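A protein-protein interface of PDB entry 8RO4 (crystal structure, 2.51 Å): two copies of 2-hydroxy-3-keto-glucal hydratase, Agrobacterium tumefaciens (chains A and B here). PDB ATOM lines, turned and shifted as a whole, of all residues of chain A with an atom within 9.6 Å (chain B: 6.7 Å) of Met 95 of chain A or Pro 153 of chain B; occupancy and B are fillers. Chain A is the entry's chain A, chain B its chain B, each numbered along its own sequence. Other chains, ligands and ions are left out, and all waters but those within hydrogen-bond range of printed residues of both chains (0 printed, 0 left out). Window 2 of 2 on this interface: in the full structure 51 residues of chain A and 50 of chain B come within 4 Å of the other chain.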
ATOM      1  N   ILE A  81       1.321 -33.830  21.773  1.00  0.00           N
ATOM      2  CA  ILE A  81       0.294 -33.562  22.778  1.00  0.00           C
ATOM      3  C   ILE A  81       0.917 -33.005  24.055  1.00  0.00           C
ATOM      4  O   ILE A  81       0.480 -31.973  24.579  1.00  0.00           O
ATOM      5  CB  ILE A  81      -0.529 -34.831  23.053  1.00  0.00           C
ATOM      6  CG1 ILE A  81      -1.267 -35.262  21.783  1.00  0.00           C
ATOM      7  CG2 ILE A  81      -1.498 -34.601  24.196  1.00  0.00           C
ATOM      8  CD1 ILE A  81      -2.271 -34.238  21.281  1.00  0.00           C
ATOM      9  N   GLN A  84       2.370 -29.495  23.835  1.00  0.00           N
ATOM     10  CA  GLN A  84       1.345 -28.459  23.818  1.00  0.00           C
ATOM     11  C   GLN A  84       0.956 -28.041  25.229  1.00  0.00           C
ATOM     12  O   GLN A  84       0.709 -26.858  25.490  1.00  0.00           O
ATOM     13  CB  GLN A  84       0.118 -28.955  23.055  1.00  0.00           C
ATOM     14  CG  GLN A  84      -0.994 -27.936  22.975  1.00  0.00           C
ATOM     15  CD  GLN A  84      -0.829 -27.012  21.791  1.00  0.00           C
ATOM     16  OE1 GLN A  84      -0.755 -27.464  20.651  1.00  0.00           O
ATOM     17  NE2 GLN A  84      -0.754 -25.712  22.056  1.00  0.00           N
ATOM     18  N   LEU A  85       0.885 -29.002  26.150  1.00  0.00           N
ATOM     19  CA  LEU A  85       0.460 -28.735  27.517  1.00  0.00           C
ATOM     20  C   LEU A  85       1.543 -28.073  28.362  1.00  0.00           C
ATOM     21  O   LEU A  85       1.264 -27.672  29.496  1.00  0.00           O
ATOM     22  CB  LEU A  85       0.004 -30.039  28.174  1.00  0.00           C
ATOM     23  CG  LEU A  85      -1.136 -30.723  27.416  1.00  0.00           C
ATOM     24  CD1 LEU A  85      -1.551 -32.024  28.088  1.00  0.00           C
ATOM     25  CD2 LEU A  85      -2.319 -29.777  27.275  1.00  0.00           C
ATOM     26  N   VAL A  88       0.027 -23.327  27.961  1.00  0.00           N
ATOM     27  CA  VAL A  88      -1.365 -23.235  27.535  1.00  0.00           C
ATOM     28  C   VAL A  88      -1.954 -21.919  28.026  1.00  0.00           C
ATOM     29  O   VAL A  88      -1.811 -21.571  29.202  1.00  0.00           O
ATOM     30  CB  VAL A  88      -2.202 -24.421  28.054  1.00  0.00           C
ATOM     31  CG1 VAL A  88      -3.650 -24.293  27.600  1.00  0.00           C
ATOM     32  CG2 VAL A  88      -1.611 -25.739  27.586  1.00  0.00           C
ATOM     33  N   HIS A  89      -2.621 -21.198  27.129  1.00  0.00           N
ATOM     34  CA  HIS A  89      -3.355 -19.997  27.501  1.00  0.00           C
ATOM     35  C   HIS A  89      -4.697 -20.383  28.128  1.00  0.00           C
ATOM     36  O   HIS A  89      -5.335 -21.341  27.679  1.00  0.00           O
ATOM     37  CB  HIS A  89      -3.578 -19.112  26.273  1.00  0.00           C
ATOM     38  CG  HIS A  89      -4.210 -17.791  26.576  1.00  0.00           C
ATOM     39  ND1 HIS A  89      -5.570 -17.637  26.746  1.00  0.00           N
ATOM     40  CD2 HIS A  89      -3.671 -16.558  26.729  1.00  0.00           C
ATOM     41  CE1 HIS A  89      -5.840 -16.370  26.997  1.00  0.00           C
ATOM     42  NE2 HIS A  89      -4.705 -15.694  26.992  1.00  0.00           N
ATOM     43  N   PRO A  90      -5.140 -19.658  29.165  1.00  0.00           N
ATOM     44  CA  PRO A  90      -6.373 -20.055  29.877  1.00  0.00           C
ATOM     45  C   PRO A  90      -7.606 -20.183  28.997  1.00  0.00           C
ATOM     46  O   PRO A  90      -8.489 -20.991  29.308  1.00  0.00           O
ATOM     47  CB  PRO A  90      -6.548 -18.935  30.911  1.00  0.00           C
ATOM     48  CG  PRO A  90      -5.171 -18.443  31.156  1.00  0.00           C
ATOM     49  CD  PRO A  90      -4.442 -18.553  29.843  1.00  0.00           C
ATOM     50  N   ALA A  91      -7.705 -19.407  27.916  1.00  0.00           N
ATOM     51  CA  ALA A  91      -8.873 -19.496  27.047  1.00  0.00           C
ATOM     52  C   ALA A  91      -9.035 -20.880  26.431  1.00  0.00           C
ATOM     53  O   ALA A  91     -10.149 -21.241  26.032  1.00  0.00           O
ATOM     54  CB  ALA A  91      -8.788 -18.437  25.946  1.00  0.00           C
ATOM     55  N   TYR A  92      -7.954 -21.659  26.340  1.00  0.00           N
ATOM     56  CA  TYR A  92      -7.989 -22.990  25.746  1.00  0.00           C
ATOM     57  C   TYR A  92      -7.808 -24.104  26.772  1.00  0.00           C
ATOM     58  O   TYR A  92      -7.627 -25.264  26.380  1.00  0.00           O
ATOM     59  CB  TYR A  92      -6.909 -23.124  24.664  1.00  0.00           C
ATOM     60  CG  TYR A  92      -6.851 -22.004  23.647  1.00  0.00           C
ATOM     61  CD1 TYR A  92      -7.836 -21.859  22.678  1.00  0.00           C
ATOM     62  CD2 TYR A  92      -5.785 -21.114  23.634  1.00  0.00           C
ATOM     63  CE1 TYR A  92      -7.772 -20.847  21.744  1.00  0.00           C
ATOM     64  CE2 TYR A  92      -5.712 -20.101  22.704  1.00  0.00           C
ATOM     65  CZ  TYR A  92      -6.706 -19.970  21.760  1.00  0.00           C
ATOM     66  OH  TYR A  92      -6.638 -18.959  20.827  1.00  0.00           O
ATOM     67  N   ASP A  93      -7.843 -23.783  28.071  1.00  0.00           N
ATOM     68  CA  ASP A  93      -7.544 -24.779  29.099  1.00  0.00           C
ATOM     69  C   ASP A  93      -8.474 -25.981  29.002  1.00  0.00           C
ATOM     70  O   ASP A  93      -8.029 -27.131  29.099  1.00  0.00           O
ATOM     71  CB  ASP A  93      -7.636 -24.143  30.486  1.00  0.00           C
ATOM     72  CG  ASP A  93      -6.293 -23.686  31.014  1.00  0.00           C
ATOM     73  OD1 ASP A  93      -5.257 -24.274  30.615  1.00  0.00           O
ATOM     74  OD2 ASP A  93      -6.270 -22.751  31.830  1.00  0.00           O
ATOM     75  N   GLU A  94      -9.773 -25.737  28.815  1.00  0.00           N
ATOM     76  CA  GLU A  94     -10.731 -26.833  28.772  1.00  0.00           C
ATOM     77  C   GLU A  94     -10.702 -27.581  27.442  1.00  0.00           C
ATOM     78  O   GLU A  94     -10.942 -28.791  27.422  1.00  0.00           O
ATOM     79  CB  GLU A  94     -12.135 -26.302  29.067  1.00  0.00           C
ATOM     80  CG  GLU A  94     -13.208 -27.370  29.095  1.00  0.00           C
ATOM     81  CD  GLU A  94     -14.520 -26.822  29.609  1.00  0.00           C
ATOM     82  OE1 GLU A  94     -14.558 -25.619  29.950  1.00  0.00           O
ATOM     83  OE2 GLU A  94     -15.516 -27.577  29.644  1.00  0.00           O
ATOM     84  N   MET A  95     -10.416 -26.897  26.327  1.00  0.00           N
ATOM     85  CA  MET A  95     -10.369 -27.591  25.044  1.00  0.00           C
ATOM     86  C   MET A  95      -9.236 -28.602  24.988  1.00  0.00           C
ATOM     87  O   MET A  95      -9.341 -29.608  24.277  1.00  0.00           O
ATOM     88  CB  MET A  95     -10.212 -26.603  23.890  1.00  0.00           C
ATOM     89  CG  MET A  95     -11.450 -25.847  23.481  1.00  0.00           C
ATOM     90  SD  MET A  95     -10.999 -24.671  22.190  1.00  0.00           S
ATOM     91  CE  MET A  95     -11.928 -25.307  20.801  1.00  0.00           C
ATOM     92  N   PHE A  96      -8.158 -28.360  25.726  1.00  0.00           N
ATOM     93  CA  PHE A  96      -7.008 -29.248  25.731  1.00  0.00           C
ATOM     94  C   PHE A  96      -7.066 -30.300  26.831  1.00  0.00           C
ATOM     95  O   PHE A  96      -6.207 -31.191  26.856  1.00  0.00           O
ATOM     96  CB  PHE A  96      -5.718 -28.435  25.875  1.00  0.00           C
ATOM     97  CG  PHE A  96      -5.213 -27.871  24.577  1.00  0.00           C
ATOM     98  CD1 PHE A  96      -5.054 -28.689  23.471  1.00  0.00           C
ATOM     99  CD2 PHE A  96      -4.896 -26.525  24.460  1.00  0.00           C
ATOM    100  CE1 PHE A  96      -4.589 -28.179  22.274  1.00  0.00           C
ATOM    101  CE2 PHE A  96      -4.431 -26.007  23.263  1.00  0.00           C
ATOM    102  CZ  PHE A  96      -4.277 -26.836  22.169  1.00  0.00           C
ATOM    103  N   ASP A  97      -8.046 -30.226  27.738  1.00  0.00           N
ATOM    104  CA  ASP A  97      -8.100 -31.191  28.830  1.00  0.00           C
ATOM    105  C   ASP A  97      -8.345 -32.601  28.314  1.00  0.00           C
ATOM    106  O   ASP A  97      -7.921 -33.572  28.949  1.00  0.00           O
ATOM    107  CB  ASP A  97      -9.177 -30.798  29.844  1.00  0.00           C
ATOM    108  CG  ASP A  97      -8.598 -30.126  31.078  1.00  0.00           C
ATOM    109  OD1 ASP A  97      -7.389 -30.301  31.342  1.00  0.00           O
ATOM    110  OD2 ASP A  97      -9.357 -29.440  31.798  1.00  0.00           O
ATOM    111  N   GLY A  98      -9.005 -32.738  27.164  1.00  0.00           N
ATOM    112  CA  GLY A  98      -9.203 -34.060  26.597  1.00  0.00           C
ATOM    113  C   GLY A  98      -7.923 -34.740  26.159  1.00  0.00           C
ATOM    114  O   GLY A  98      -7.944 -35.940  25.861  1.00  0.00           O
ATOM    115  N   PHE A  99      -6.816 -34.004  26.127  1.00  0.00           N
ATOM    116  CA  PHE A  99      -5.517 -34.530  25.744  1.00  0.00           C
ATOM    117  C   PHE A  99      -4.656 -34.886  26.947  1.00  0.00           C
ATOM    118  O   PHE A  99      -3.588 -35.483  26.774  1.00  0.00           O
ATOM    119  CB  PHE A  99      -4.787 -33.514  24.859  1.00  0.00           C
ATOM    120  CG  PHE A  99      -5.343 -33.422  23.468  1.00  0.00           C
ATOM    121  CD1 PHE A  99      -5.930 -34.529  22.871  1.00  0.00           C
ATOM    122  CD2 PHE A  99      -5.296 -32.230  22.765  1.00  0.00           C
ATOM    123  CE1 PHE A  99      -6.449 -34.453  21.593  1.00  0.00           C
ATOM    124  CE2 PHE A  99      -5.814 -32.146  21.485  1.00  0.00           C
ATOM    125  CZ  PHE A  99      -6.392 -33.259  20.898  1.00  0.00           C
ATOM    126  N   ALA A 100      -5.088 -34.528  28.148  1.00  0.00           N
ATOM    127  CA  ALA A 100      -4.425 -34.838  29.401  1.00  0.00           C
ATOM    128  C   ALA A 100      -5.096 -36.029  30.066  1.00  0.00           C
ATOM    129  O   ALA A 100      -6.240 -36.367  29.747  1.00  0.00           O
ATOM    130  CB  ALA A 100      -4.473 -33.627  30.340  1.00  0.00           C
ATOM    131  N   ARG A 105      -7.609 -33.421  34.597  1.00  0.00           N
ATOM    132  CA  ARG A 105      -8.542 -32.453  34.035  1.00  0.00           C
ATOM    133  C   ARG A 105      -9.076 -31.533  35.127  1.00  0.00           C
ATOM    134  O   ARG A 105      -9.421 -31.976  36.227  1.00  0.00           O
ATOM    135  CB  ARG A 105      -9.697 -33.168  33.333  1.00  0.00           C
ATOM    136  CG  ARG A 105      -9.264 -34.214  32.315  1.00  0.00           C
ATOM    137  CD  ARG A 105     -10.295 -34.352  31.207  1.00  0.00           C
ATOM    138  NE  ARG A 105     -10.571 -35.742  30.865  1.00  0.00           N
ATOM    139  CZ  ARG A 105      -9.845 -36.469  30.026  1.00  0.00           C
ATOM    140  NH1 ARG A 105      -8.764 -35.978  29.445  1.00  0.00           N
ATOM    141  NH2 ARG A 105     -10.213 -37.720  29.763  1.00  0.00           N
ATOM    142  N   GLY A 106      -9.140 -30.239  34.818  1.00  0.00           N
ATOM    143  CA  GLY A 106      -9.558 -29.238  35.776  1.00  0.00           C
ATOM    144  C   GLY A 106      -8.468 -28.727  36.691  1.00  0.00           C
ATOM    145  O   GLY A 106      -8.749 -27.866  37.537  1.00  0.00           O
ATOM    146  N   ARG A 111      -1.443 -30.400  35.424  1.00  0.00           N
ATOM    147  CA  ARG A 111      -1.328 -30.844  34.038  1.00  0.00           C
ATOM    148  C   ARG A 111      -0.022 -30.377  33.410  1.00  0.00           C
ATOM    149  O   ARG A 111       0.628 -31.130  32.674  1.00  0.00           O
ATOM    150  CB  ARG A 111      -2.517 -30.332  33.228  1.00  0.00           C
ATOM    151  CG  ARG A 111      -2.609 -30.896  31.826  1.00  0.00           C
ATOM    152  CD  ARG A 111      -3.636 -30.130  31.009  1.00  0.00           C
ATOM    153  NE  ARG A 111      -3.331 -28.704  30.975  1.00  0.00           N
ATOM    154  CZ  ARG A 111      -4.163 -27.766  30.540  1.00  0.00           C
ATOM    155  NH1 ARG A 111      -5.375 -28.066  30.100  1.00  0.00           N
ATOM    156  NH2 ARG A 111      -3.770 -26.495  30.552  1.00  0.00           N
ATOM    157  N   TYR A 260     -14.185 -19.684   9.813  1.00  0.00           N
ATOM    158  CA  TYR A 260     -14.717 -20.757  10.654  1.00  0.00           C
ATOM    159  C   TYR A 260     -15.260 -21.933   9.846  1.00  0.00           C
ATOM    160  O   TYR A 260     -16.035 -22.739  10.369  1.00  0.00           O
ATOM    161  CB  TYR A 260     -15.806 -20.240  11.608  1.00  0.00           C
ATOM    162  CG  TYR A 260     -15.385 -19.060  12.448  1.00  0.00           C
ATOM    163  CD1 TYR A 260     -14.474 -19.214  13.487  1.00  0.00           C
ATOM    164  CD2 TYR A 260     -15.904 -17.792  12.213  1.00  0.00           C
ATOM    165  CE1 TYR A 260     -14.081 -18.139  14.263  1.00  0.00           C
ATOM    166  CE2 TYR A 260     -15.517 -16.708  12.985  1.00  0.00           C
ATOM    167  CZ  TYR A 260     -14.606 -16.889  14.009  1.00  0.00           C
ATOM    168  OH  TYR A 260     -14.216 -15.819  14.780  1.00  0.00           O
ATOM    169  N   PHE B 145     -10.716 -18.869  18.395  1.00  0.00           N
ATOM    170  CA  PHE B 145     -10.821 -20.197  17.803  1.00  0.00           C
ATOM    171  C   PHE B 145     -10.839 -20.143  16.278  1.00  0.00           C
ATOM    172  O   PHE B 145     -11.452 -20.993  15.626  1.00  0.00           O
ATOM    173  CB  PHE B 145     -12.060 -20.909  18.347  1.00  0.00           C
ATOM    174  CG  PHE B 145     -12.272 -20.701  19.824  1.00  0.00           C
ATOM    175  CD1 PHE B 145     -11.417 -21.282  20.749  1.00  0.00           C
ATOM    176  CD2 PHE B 145     -13.302 -19.895  20.286  1.00  0.00           C
ATOM    177  CE1 PHE B 145     -11.598 -21.079  22.109  1.00  0.00           C
ATOM    178  CE2 PHE B 145     -13.488 -19.686  21.646  1.00  0.00           C
ATOM    179  CZ  PHE B 145     -12.635 -20.278  22.556  1.00  0.00           C
ATOM    180  N   TRP B 149      -7.281 -25.535  15.844  1.00  0.00           N
ATOM    181  CA  TRP B 149      -6.366 -26.241  16.735  1.00  0.00           C
ATOM    182  C   TRP B 149      -6.286 -25.511  18.071  1.00  0.00           C
ATOM    183  O   TRP B 149      -5.751 -24.397  18.140  1.00  0.00           O
ATOM    184  CB  TRP B 149      -4.972 -26.376  16.121  1.00  0.00           C
ATOM    185  CG  TRP B 149      -4.036 -27.133  17.007  1.00  0.00           C
ATOM    186  CD1 TRP B 149      -3.037 -26.615  17.776  1.00  0.00           C
ATOM    187  CD2 TRP B 149      -4.016 -28.550  17.224  1.00  0.00           C
ATOM    188  NE1 TRP B 149      -2.395 -27.619  18.459  1.00  0.00           N
ATOM    189  CE2 TRP B 149      -2.976 -28.817  18.136  1.00  0.00           C
ATOM    190  CE3 TRP B 149      -4.773 -29.617  16.732  1.00  0.00           C
ATOM    191  CZ2 TRP B 149      -2.674 -30.107  18.567  1.00  0.00           C
ATOM    192  CZ3 TRP B 149      -4.473 -30.897  17.161  1.00  0.00           C
ATOM    193  CH2 TRP B 149      -3.431 -31.131  18.070  1.00  0.00           C
ATOM    194  N   PRO B 150      -6.808 -26.100  19.157  1.00  0.00           N
ATOM    195  CA  PRO B 150      -7.412 -27.441  19.261  1.00  0.00           C
ATOM    196  C   PRO B 150      -8.703 -27.580  18.457  1.00  0.00           C
ATOM    197  O   PRO B 150      -9.347 -26.586  18.132  1.00  0.00           O
ATOM    198  CB  PRO B 150      -7.654 -27.589  20.770  1.00  0.00           C
ATOM    199  CG  PRO B 150      -7.845 -26.184  21.257  1.00  0.00           C
ATOM    200  CD  PRO B 150      -6.901 -25.356  20.427  1.00  0.00           C
ATOM    201  N   GLN B 151      -9.081 -28.810  18.119  1.00  0.00           N
ATOM    202  CA  GLN B 151     -10.235 -29.038  17.261  1.00  0.00           C
ATOM    203  C   GLN B 151     -11.502 -28.470  17.892  1.00  0.00           C
ATOM    204  O   GLN B 151     -11.734 -28.605  19.097  1.00  0.00           O
ATOM    205  CB  GLN B 151     -10.392 -30.536  16.993  1.00  0.00           C
ATOM    206  CG  GLN B 151     -11.272 -30.874  15.804  1.00  0.00           C
ATOM    207  CD  GLN B 151     -11.152 -32.331  15.392  1.00  0.00           C
ATOM    208  OE1 GLN B 151     -10.784 -33.188  16.196  1.00  0.00           O
ATOM    209  NE2 GLN B 151     -11.455 -32.615  14.130  1.00  0.00           N
ATOM    210  N   ARG B 152     -12.322 -27.822  17.070  1.00  0.00           N
ATOM    211  CA  ARG B 152     -13.503 -27.129  17.577  1.00  0.00           C
ATOM    212  C   ARG B 152     -14.616 -28.121  17.893  1.00  0.00           C
ATOM    213  O   ARG B 152     -14.936 -28.971  17.056  1.00  0.00           O
ATOM    214  CB  ARG B 152     -14.018 -26.104  16.573  1.00  0.00           C
ATOM    215  CG  ARG B 152     -13.169 -24.866  16.422  1.00  0.00           C
ATOM    216  CD  ARG B 152     -13.857 -23.906  15.473  1.00  0.00           C
ATOM    217  NE  ARG B 152     -12.915 -23.087  14.723  1.00  0.00           N
ATOM    218  CZ  ARG B 152     -12.703 -23.204  13.420  1.00  0.00           C
ATOM    219  NH1 ARG B 152     -13.340 -24.111  12.697  1.00  0.00           N
ATOM    220  NH2 ARG B 152     -11.838 -22.386  12.828  1.00  0.00           N
ATOM    221  N   PRO B 153     -15.219 -28.047  19.077  1.00  0.00           N
ATOM    222  CA  PRO B 153     -16.356 -28.917  19.383  1.00  0.00           C
ATOM    223  C   PRO B 153     -17.555 -28.574  18.513  1.00  0.00           C
ATOM    224  O   PRO B 153     -17.697 -27.459  18.006  1.00  0.00           O
ATOM    225  CB  PRO B 153     -16.650 -28.625  20.859  1.00  0.00           C
ATOM    226  CG  PRO B 153     -15.456 -27.889  21.372  1.00  0.00           C
ATOM    227  CD  PRO B 153     -14.878 -27.165  20.204  1.00  0.00           C
ATOM    228  N   ALA B 154     -18.426 -29.564  18.340  1.00  0.00           N
ATOM    229  CA  ALA B 154     -19.617 -29.370  17.527  1.00  0.00           C
ATOM    230  C   ALA B 154     -20.527 -28.329  18.165  1.00  0.00           C
ATOM    231  O   ALA B 154     -20.770 -28.357  19.375  1.00  0.00           O
ATOM    232  CB  ALA B 154     -20.362 -30.694  17.353  1.00  0.00           C
ATOM    233  N   GLY B 155     -21.022 -27.401  17.346  1.00  0.00           N
ATOM    234  CA  GLY B 155     -21.940 -26.380  17.803  1.00  0.00           C
ATOM    235  C   GLY B 155     -21.303 -25.112  18.335  1.00  0.00           C
ATOM    236  O   GLY B 155     -22.028 -24.145  18.607  1.00  0.00           O
ATOM    237  N   LEU B 156     -19.978 -25.076  18.487  1.00  0.00           N
ATOM    238  CA  LEU B 156     -19.332 -23.888  19.035  1.00  0.00           C
ATOM    239  C   LEU B 156     -19.522 -22.688  18.114  1.00  0.00           C
ATOM    240  O   LEU B 156     -19.927 -21.607  18.558  1.00  0.00           O
ATOM    241  CB  LEU B 156     -17.847 -24.153  19.274  1.00  0.00           C
ATOM    242  CG  LEU B 156     -17.112 -22.997  19.955  1.00  0.00           C
ATOM    243  CD1 LEU B 156     -17.666 -22.770  21.350  1.00  0.00           C
ATOM    244  CD2 LEU B 156     -15.615 -23.260  20.007  1.00  0.00           C
ATOM    245  N   VAL B 157     -19.225 -22.858  16.825  1.00  0.00           N
ATOM    246  CA  VAL B 157     -19.366 -21.756  15.878  1.00  0.00           C
ATOM    247  C   VAL B 157     -20.829 -21.361  15.725  1.00  0.00           C
ATOM    248  O   VAL B 157     -21.166 -20.170  15.721  1.00  0.00           O
ATOM    249  CB  VAL B 157     -18.737 -22.133  14.526  1.00  0.00           C
ATOM    250  CG1 VAL B 157     -19.082 -21.095  13.472  1.00  0.00           C
ATOM    251  CG2 VAL B 157     -17.227 -22.265  14.669  1.00  0.00           C
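No position is printed for both chains.
Of the 9 pairs that touch across the chains among the printed residues, none has its exchanged pair printed and touching as well.
CE1 of Tyr 92 of chain A touches CD1 of Phe 145 of chain B, at 3.8 Å.
SD of Met 95 of chain A touches CE1 of Phe 145 of chain B (3.6 Å).
Met 95 of chain A touches Pro 150 of chain B (CB to CG, 3.6 Å).
Met 95 of chain A touches Gln 151 of chain B (CE to O, 3.7 Å).
CD of Pro 153 of chain B touches CE of Met 95 of chain A (3.5 Å).
Phe 96 of chain A touches Pro 150 of chain B (CE1 to CB, 3.5 Å).
Tyr 260 of chain A touches Arg 152 of chain B.
Val 157 of chain B touches Tyr 260 of chain A (CG1 to CB, 3.9 Å).
The guanidinium group (NE) of Arg 152 of chain B lies within hydrogen-bond range of the backbone carbonyl oxygen (O) of Phe 145 of chain B, at 2.7 Å.
The indole nitrogen of Trp 149 of chain B sits at hydrogen-bond distance from the side-chain amide oxygen of Gln 84 of chain A (2.7 Å).
Of chain B, only Phe 145, Pro 150, Gln 151 and Pro 153 come within 4 Å of Met 95 of chain A.
Of chain A, only Met 95 comes within 4 Å of Pro 153 of chain B.
Of chain A, only Met 95 and Phe 96 come within 4 Å of Pro 150 of chain B.
No residue of chain A comes within 4 Å of Ala 154 of chain B.
No residue of chain A comes within 4 Å of Gly 155 of chain B.
Printed residues of chain A within 4 Å of Arg 152 of chain B: Tyr 260 (3.8 Å).
Printed residues of chain A within 4 Å of Gln 151 of chain B: Met 95 (3.7 Å).
Of the printed residues of chain B, Tyr 92 of chain A touches Phe 145 (3.8 Å).
Printed residues of chain A within 4 Å of Phe 145 of chain B: Tyr 92 and Met 95.
Printed residues of chain A within 4 Å of Trp 149 of chain B: Gln 84 (2.7 Å).
Gly 98 of chain A touches none of the printed residues of chain B.
The nearest printed residue of chain A that does not touch Val 157 of chain B is Met 95 of chain A (8.7 Å).
Of the 20 printed residues of chain A, 5 touch a printed residue of chain B.
Printed residues of chain A that touch a printed residue of chain B: Gln 84, Tyr 92, Met 95, Phe 96 and Tyr 260.
Hydrophobic or aromatic side chains of chain A that line the printed part of chain B: Tyr 92, Met 95, Phe 96 and Tyr 260.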
